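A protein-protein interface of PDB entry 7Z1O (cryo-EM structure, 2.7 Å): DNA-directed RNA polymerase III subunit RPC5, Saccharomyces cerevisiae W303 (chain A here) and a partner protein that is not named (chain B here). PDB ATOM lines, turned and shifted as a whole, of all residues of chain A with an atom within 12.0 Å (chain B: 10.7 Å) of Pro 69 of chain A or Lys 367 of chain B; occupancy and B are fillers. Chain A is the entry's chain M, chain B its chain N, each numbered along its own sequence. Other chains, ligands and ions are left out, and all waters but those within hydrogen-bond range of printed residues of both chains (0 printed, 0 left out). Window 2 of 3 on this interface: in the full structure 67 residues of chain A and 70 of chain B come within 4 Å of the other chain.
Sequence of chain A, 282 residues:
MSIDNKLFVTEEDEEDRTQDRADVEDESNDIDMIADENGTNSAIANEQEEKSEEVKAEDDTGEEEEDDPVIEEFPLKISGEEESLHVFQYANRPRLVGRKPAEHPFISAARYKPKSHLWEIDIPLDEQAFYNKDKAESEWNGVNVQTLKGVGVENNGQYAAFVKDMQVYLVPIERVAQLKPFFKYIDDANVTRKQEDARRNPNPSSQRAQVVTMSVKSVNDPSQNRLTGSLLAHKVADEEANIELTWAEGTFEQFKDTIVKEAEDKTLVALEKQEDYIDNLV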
ATOM      1  N   ASP A  68      -2.434  14.952 -11.192  1.00  0.00           N
ATOM      2  CA  ASP A  68      -2.790  13.535 -11.125  1.00  0.00           C
ATOM      3  C   ASP A  68      -3.315  12.933 -12.452  1.00  0.00           C
ATOM      4  O   ASP A  68      -3.002  11.777 -12.740  1.00  0.00           O
ATOM      5  CB  ASP A  68      -3.808  13.296  -9.999  1.00  0.00           C
ATOM      6  CG  ASP A  68      -3.410  13.968  -8.699  1.00  0.00           C
ATOM      7  OD1 ASP A  68      -2.196  14.127  -8.457  1.00  0.00           O
ATOM      8  OD2 ASP A  68      -4.314  14.338  -7.918  1.00  0.00           O
ATOM      9  N   PRO A  69      -4.113  13.665 -13.247  1.00  0.00           N
ATOM     10  CA  PRO A  69      -4.404  13.178 -14.602  1.00  0.00           C
ATOM     11  C   PRO A  69      -3.144  13.061 -15.447  1.00  0.00           C
ATOM     12  O   PRO A  69      -2.198  13.839 -15.305  1.00  0.00           O
ATOM     13  CB  PRO A  69      -5.359  14.235 -15.162  1.00  0.00           C
ATOM     14  CG  PRO A  69      -6.064  14.738 -13.987  1.00  0.00           C
ATOM     15  CD  PRO A  69      -5.047  14.754 -12.884  1.00  0.00           C
ATOM     16  N   VAL A  70      -3.144  12.072 -16.333  1.00  0.00           N
ATOM     17  CA  VAL A  70      -2.018  11.792 -17.215  1.00  0.00           C
ATOM     18  C   VAL A  70      -2.200  12.562 -18.514  1.00  0.00           C
ATOM     19  O   VAL A  70      -3.300  12.605 -19.079  1.00  0.00           O
ATOM     20  CB  VAL A  70      -1.900  10.280 -17.476  1.00  0.00           C
ATOM     21  CG1 VAL A  70      -0.621   9.969 -18.226  1.00  0.00           C
ATOM     22  CG2 VAL A  70      -1.957   9.511 -16.165  1.00  0.00           C
ATOM     23  N   ILE A  71      -1.119  13.174 -18.996  1.00  0.00           N
ATOM     24  CA  ILE A  71      -1.171  13.970 -20.217  1.00  0.00           C
ATOM     25  C   ILE A  71      -0.682  13.148 -21.404  1.00  0.00           C
ATOM     26  O   ILE A  71      -1.096  13.383 -22.545  1.00  0.00           O
ATOM     27  CB  ILE A  71      -0.361  15.271 -20.071  1.00  0.00           C
ATOM     28  CG1 ILE A  71       1.075  14.971 -19.637  1.00  0.00           C
ATOM     29  CG2 ILE A  71      -1.032  16.207 -19.079  1.00  0.00           C
ATOM     30  CD1 ILE A  71       2.007  16.157 -19.749  1.00  0.00           C
ATOM     31  N   GLU A  72       0.199  12.180 -21.149  1.00  0.00           N
ATOM     32  CA  GLU A  72       0.727  11.343 -22.217  1.00  0.00           C
ATOM     33  C   GLU A  72       1.183  10.011 -21.640  1.00  0.00           C
ATOM     34  O   GLU A  72       1.717   9.958 -20.530  1.00  0.00           O
ATOM     35  CB  GLU A  72       1.887  12.032 -22.945  1.00  0.00           C
ATOM     36  CG  GLU A  72       2.961  12.582 -22.024  1.00  0.00           C
ATOM     37  CD  GLU A  72       4.161  13.117 -22.780  1.00  0.00           C
ATOM     38  OE1 GLU A  72       4.218  12.933 -24.014  1.00  0.00           O
ATOM     39  OE2 GLU A  72       5.044  13.723 -22.139  1.00  0.00           O
ATOM     40  N   GLU A  73       0.974   8.942 -22.406  1.00  0.00           N
ATOM     41  CA  GLU A  73       1.387   7.602 -22.016  1.00  0.00           C
ATOM     42  C   GLU A  73       2.168   6.965 -23.156  1.00  0.00           C
ATOM     43  O   GLU A  73       1.856   7.179 -24.331  1.00  0.00           O
ATOM     44  CB  GLU A  73       0.175   6.733 -21.633  1.00  0.00           C
ATOM     45  CG  GLU A  73      -0.885   6.585 -22.715  1.00  0.00           C
ATOM     46  CD  GLU A  73      -0.666   5.363 -23.584  1.00  0.00           C
ATOM     47  OE1 GLU A  73       0.048   4.438 -23.142  1.00  0.00           O
ATOM     48  OE2 GLU A  73      -1.205   5.329 -24.710  1.00  0.00           O
ATOM     49  N   PHE A  74       3.194   6.191 -22.803  1.00  0.00           N
ATOM     50  CA  PHE A  74       4.045   5.527 -23.782  1.00  0.00           C
ATOM     51  C   PHE A  74       3.911   4.021 -23.630  1.00  0.00           C
ATOM     52  O   PHE A  74       4.183   3.495 -22.541  1.00  0.00           O
ATOM     53  CB  PHE A  74       5.502   5.947 -23.610  1.00  0.00           C
ATOM     54  CG  PHE A  74       5.692   7.424 -23.421  1.00  0.00           C
ATOM     55  CD1 PHE A  74       5.081   8.329 -24.273  1.00  0.00           C
ATOM     56  CD2 PHE A  74       6.486   7.905 -22.394  1.00  0.00           C
ATOM     57  CE1 PHE A  74       5.252   9.687 -24.100  1.00  0.00           C
ATOM     58  CE2 PHE A  74       6.668   9.261 -22.217  1.00  0.00           C
ATOM     59  CZ  PHE A  74       6.049  10.155 -23.070  1.00  0.00           C
ATOM     60  N   ASN B 284      12.804  13.974  -8.784  1.00  0.00           N
ATOM     61  CA  ASN B 284      12.209  14.812  -9.823  1.00  0.00           C
ATOM     62  C   ASN B 284      13.197  15.081 -10.954  1.00  0.00           C
ATOM     63  O   ASN B 284      12.833  15.026 -12.140  1.00  0.00           O
ATOM     64  CB  ASN B 284      11.708  16.126  -9.223  1.00  0.00           C
ATOM     65  CG  ASN B 284      10.442  15.949  -8.410  1.00  0.00           C
ATOM     66  OD1 ASN B 284      10.415  16.230  -7.212  1.00  0.00           O
ATOM     67  ND2 ASN B 284       9.384  15.479  -9.058  1.00  0.00           N
ATOM     68  N   HIS B 287      13.454  11.955 -12.986  1.00  0.00           N
ATOM     69  CA  HIS B 287      12.277  11.781 -13.833  1.00  0.00           C
ATOM     70  C   HIS B 287      12.364  12.649 -15.083  1.00  0.00           C
ATOM     71  O   HIS B 287      12.070  12.188 -16.195  1.00  0.00           O
ATOM     72  CB  HIS B 287      11.008  12.111 -13.047  1.00  0.00           C
ATOM     73  CG  HIS B 287      10.579  11.027 -12.107  1.00  0.00           C
ATOM     74  ND1 HIS B 287       9.645  11.231 -11.116  1.00  0.00           N
ATOM     75  CD2 HIS B 287      10.954   9.730 -12.011  1.00  0.00           C
ATOM     76  CE1 HIS B 287       9.464  10.106 -10.447  1.00  0.00           C
ATOM     77  NE2 HIS B 287      10.246   9.180 -10.969  1.00  0.00           N
ATOM     78  N   GLN B 288      12.783  13.909 -14.917  1.00  0.00           N
ATOM     79  CA  GLN B 288      12.957  14.785 -16.073  1.00  0.00           C
ATOM     80  C   GLN B 288      14.033  14.254 -17.016  1.00  0.00           C
ATOM     81  O   GLN B 288      13.855  14.265 -18.242  1.00  0.00           O
ATOM     82  CB  GLN B 288      13.300  16.201 -15.614  1.00  0.00           C
ATOM     83  CG  GLN B 288      12.159  16.919 -14.917  1.00  0.00           C
ATOM     84  CD  GLN B 288      12.506  18.351 -14.560  1.00  0.00           C
ATOM     85  OE1 GLN B 288      13.663  18.674 -14.298  1.00  0.00           O
ATOM     86  NE2 GLN B 288      11.499  19.217 -14.549  1.00  0.00           N
ATOM     87  N   LEU B 291      12.663  11.212 -18.943  1.00  0.00           N
ATOM     88  CA  LEU B 291      11.767  11.624 -20.021  1.00  0.00           C
ATOM     89  C   LEU B 291      12.545  12.206 -21.197  1.00  0.00           C
ATOM     90  O   LEU B 291      12.270  11.876 -22.361  1.00  0.00           O
ATOM     91  CB  LEU B 291      10.747  12.634 -19.501  1.00  0.00           C
ATOM     92  CG  LEU B 291       9.683  13.080 -20.502  1.00  0.00           C
ATOM     93  CD1 LEU B 291       8.935  11.877 -21.052  1.00  0.00           C
ATOM     94  CD2 LEU B 291       8.723  14.067 -19.861  1.00  0.00           C
ATOM     95  N   ARG B 364       3.763   6.532 -17.980  1.00  0.00           N
ATOM     96  CA  ARG B 364       2.852   7.662 -17.941  1.00  0.00           C
ATOM     97  C   ARG B 364       3.546   8.868 -17.328  1.00  0.00           C
ATOM     98  O   ARG B 364       4.229   8.754 -16.306  1.00  0.00           O
ATOM     99  CB  ARG B 364       1.596   7.309 -17.141  1.00  0.00           C
ATOM    100  CG  ARG B 364       1.112   5.885 -17.356  1.00  0.00           C
ATOM    101  CD  ARG B 364       0.002   5.519 -16.388  1.00  0.00           C
ATOM    102  NE  ARG B 364       0.346   5.857 -15.013  1.00  0.00           N
ATOM    103  CZ  ARG B 364      -0.510   5.844 -14.002  1.00  0.00           C
ATOM    104  NH1 ARG B 364      -1.779   5.510 -14.174  1.00  0.00           N
ATOM    105  NH2 ARG B 364      -0.085   6.175 -12.787  1.00  0.00           N
ATOM    106  N   VAL B 365       3.364  10.025 -17.962  1.00  0.00           N
ATOM    107  CA  VAL B 365       3.941  11.285 -17.510  1.00  0.00           C
ATOM    108  C   VAL B 365       2.807  12.179 -17.036  1.00  0.00           C
ATOM    109  O   VAL B 365       1.818  12.374 -17.753  1.00  0.00           O
ATOM    110  CB  VAL B 365       4.755  11.967 -18.619  1.00  0.00           C
ATOM    111  CG1 VAL B 365       5.491  13.175 -18.065  1.00  0.00           C
ATOM    112  CG2 VAL B 365       5.734  10.985 -19.228  1.00  0.00           C
ATOM    113  N   HIS B 366       2.946  12.718 -15.831  1.00  0.00           N
ATOM    114  CA  HIS B 366       1.947  13.603 -15.258  1.00  0.00           C
ATOM    115  C   HIS B 366       2.323  15.060 -15.514  1.00  0.00           C
ATOM    116  O   HIS B 366       3.370  15.366 -16.090  1.00  0.00           O
ATOM    117  CB  HIS B 366       1.796  13.326 -13.763  1.00  0.00           C
ATOM    118  CG  HIS B 366       1.370  11.924 -13.455  1.00  0.00           C
ATOM    119  ND1 HIS B 366       2.202  11.010 -12.845  1.00  0.00           N
ATOM    120  CD2 HIS B 366       0.204  11.276 -13.685  1.00  0.00           C
ATOM    121  CE1 HIS B 366       1.565   9.862 -12.708  1.00  0.00           C
ATOM    122  NE2 HIS B 366       0.351   9.997 -13.209  1.00  0.00           N
ATOM    123  N   LYS B 367       1.447  15.971 -15.083  1.00  0.00           N
ATOM    124  CA  LYS B 367       1.684  17.389 -15.338  1.00  0.00           C
ATOM    125  C   LYS B 367       2.823  17.926 -14.480  1.00  0.00           C
ATOM    126  O   LYS B 367       3.501  18.886 -14.865  1.00  0.00           O
ATOM    127  CB  LYS B 367       0.406  18.197 -15.102  1.00  0.00           C
ATOM    128  CG  LYS B 367      -0.079  18.219 -13.661  1.00  0.00           C
ATOM    129  CD  LYS B 367      -1.304  19.105 -13.509  1.00  0.00           C
ATOM    130  CE  LYS B 367      -2.527  18.465 -14.137  1.00  0.00           C
ATOM    131  NZ  LYS B 367      -2.914  17.228 -13.410  1.00  0.00           N
ATOM    132  N   SER B 368       3.052  17.319 -13.313  1.00  0.00           N
ATOM    133  CA  SER B 368       4.121  17.779 -12.435  1.00  0.00           C
ATOM    134  C   SER B 368       5.497  17.371 -12.938  1.00  0.00           C
ATOM    135  O   SER B 368       6.506  17.855 -12.414  1.00  0.00           O
ATOM    136  CB  SER B 368       3.904  17.246 -11.018  1.00  0.00           C
ATOM    137  OG  SER B 368       3.766  15.836 -11.020  1.00  0.00           O
ATOM    138  N   GLY B 369       5.563  16.498 -13.939  1.00  0.00           N
ATOM    139  CA  GLY B 369       6.821  16.010 -14.460  1.00  0.00           C
ATOM    140  C   GLY B 369       7.229  14.644 -13.959  1.00  0.00           C
ATOM    141  O   GLY B 369       8.193  14.074 -14.485  1.00  0.00           O
ATOM    142  N   LYS B 370       6.536  14.104 -12.960  1.00  0.00           N
ATOM    143  CA  LYS B 370       6.863  12.778 -12.459  1.00  0.00           C
ATOM    144  C   LYS B 370       6.416  11.710 -13.447  1.00  0.00           C
ATOM    145  O   LYS B 370       5.485  11.913 -14.231  1.00  0.00           O
ATOM    146  CB  LYS B 370       6.211  12.546 -11.096  1.00  0.00           C
ATOM    147  CG  LYS B 370       4.694  12.537 -11.118  1.00  0.00           C
ATOM    148  CD  LYS B 370       4.128  12.300  -9.729  1.00  0.00           C
ATOM    149  CE  LYS B 370       4.390  10.878  -9.263  1.00  0.00           C
ATOM    150  NZ  LYS B 370       3.647   9.881 -10.082  1.00  0.00           N
ATOM    151  N   LEU B 371       7.093  10.568 -13.410  1.00  0.00           N
ATOM    152  CA  LEU B 371       6.810   9.450 -14.297  1.00  0.00           C
ATOM    153  C   LEU B 371       6.402   8.237 -13.471  1.00  0.00           C
ATOM    154  O   LEU B 371       6.926   8.016 -12.376  1.00  0.00           O
ATOM    155  CB  LEU B 371       8.030   9.113 -15.158  1.00  0.00           C
ATOM    156  CG  LEU B 371       8.172   9.814 -16.509  1.00  0.00           C
ATOM    157  CD1 LEU B 371       8.637  11.250 -16.330  1.00  0.00           C
ATOM    158  CD2 LEU B 371       9.132   9.046 -17.401  1.00  0.00           C
ATOM    159  N   SER B 372       5.457   7.459 -13.993  1.00  0.00           N
ATOM    160  CA  SER B 372       4.991   6.254 -13.318  1.00  0.00           C
ATOM    161  C   SER B 372       4.837   5.138 -14.338  1.00  0.00           C
ATOM    162  O   SER B 372       4.288   5.359 -15.420  1.00  0.00           O
ATOM    163  CB  SER B 372       3.662   6.500 -12.597  1.00  0.00           C
ATOM    164  OG  SER B 372       2.622   6.764 -13.522  1.00  0.00           O
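Asp 68 of chain A touches just these residues of chain B: His 366 (3.4 Å) and Lys 367 (3.2 Å).
Of the printed residues of chain B, Ile 71 of chain A touches Val 365 and His 366.
Of the printed residues of chain B, Glu 72 of chain A touches Arg 364 and Val 365.
Printed residues of chain B within 4 Å of Phe 74 of chain A: Leu 291 and Val 365.
Asn 284 of chain B touches none of the printed residues of chain A.
Printed residues of chain A within 4 Å of Leu 291 of chain B: Phe 74.
Of the printed residues of chain A, Arg 364 of chain B touches Val 70 and Glu 72.
Of chain A, only Asp 68 and Pro 69 come within 4 Å of Lys 367 of chain B.
No residue of chain A comes within 4 Å of Ser 368 of chain B.
The nearest residue of chain A that does not touch Lys 367 of chain B is Ile 71 of chain A (4.6 Å).
The nearest printed residue of chain A that does not touch Arg 364 of chain B is Glu 73 of chain A (4.3 Å).
Of the 7 printed residues of chain A, 6 touch a printed residue of chain B.
Printed residues of chain A that touch a printed residue of chain B: Asp 68, Pro 69, Val 70, Ile 71, Glu 72 and Phe 74.
Hydrophobic or aromatic side chains of chain A that line the printed part of chain B: Pro 69, Val 70, Ile 71 and Phe 74.
Along chain A the printed residues that touch a printed residue of chain B span positions 68 to 74.
Among the printed residues, no Asp or Glu carboxylate lies within 4 Å of a Lys or Arg side-chain nitrogen of the other chain.
His 366 of chain B touches Asp 68 of chain A (CD2 to O, 3.4 Å).
O of Pro 69 of chain A touches CD2 of His 366 of chain B, 3.9 Å away.
NZ of Lys 367 of chain B touches CD of Pro 69 of chain A, 3.3 Å away.
Arg 364 of chain B touches Val 70 of chain A.
Val 70 of chain A touches Val 365 of chain B (CG1 to O, 3.5 Å).
CD2 of His 366 of chain B touches CG2 of Val 70 of chain A, at 3.7 Å.
Ile 71 of chain A touches His 366 of chain B.
O of Glu 72 of chain A touches CA of Arg 364 of chain B, 3.6 Å away.
Phe 74 of chain A touches Leu 291 of chain B (CE2 to CD1, 3.7 Å).
CE2 of Phe 74 of chain A touches CG2 of Val 365 of chain B, at 3.6 Å.
The backbone carbonyl oxygen (O) of Ser 372 of chain B is in hydrogen-bond range of the backbone NH (N) of Arg 364 of chain B (2.9 Å).
NZ of Lys 370 of chain B lies within hydrogen-bond range of ND1 of His 366 of chain B (3.3 Å).
N of Ile 71 of chain A sits at hydrogen-bond distance from O of Val 365 of chain B.
The backbone carbonyl oxygen of Glu 72 of chain A is in hydrogen-bond range of the backbone NH of Val 365 of chain B (3.1 Å).
The backbone NH (N) of Asp 68 of chain A lies close to the side-chain amino group (NZ) of Lys 367 of chain B, 3.2 Å away.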
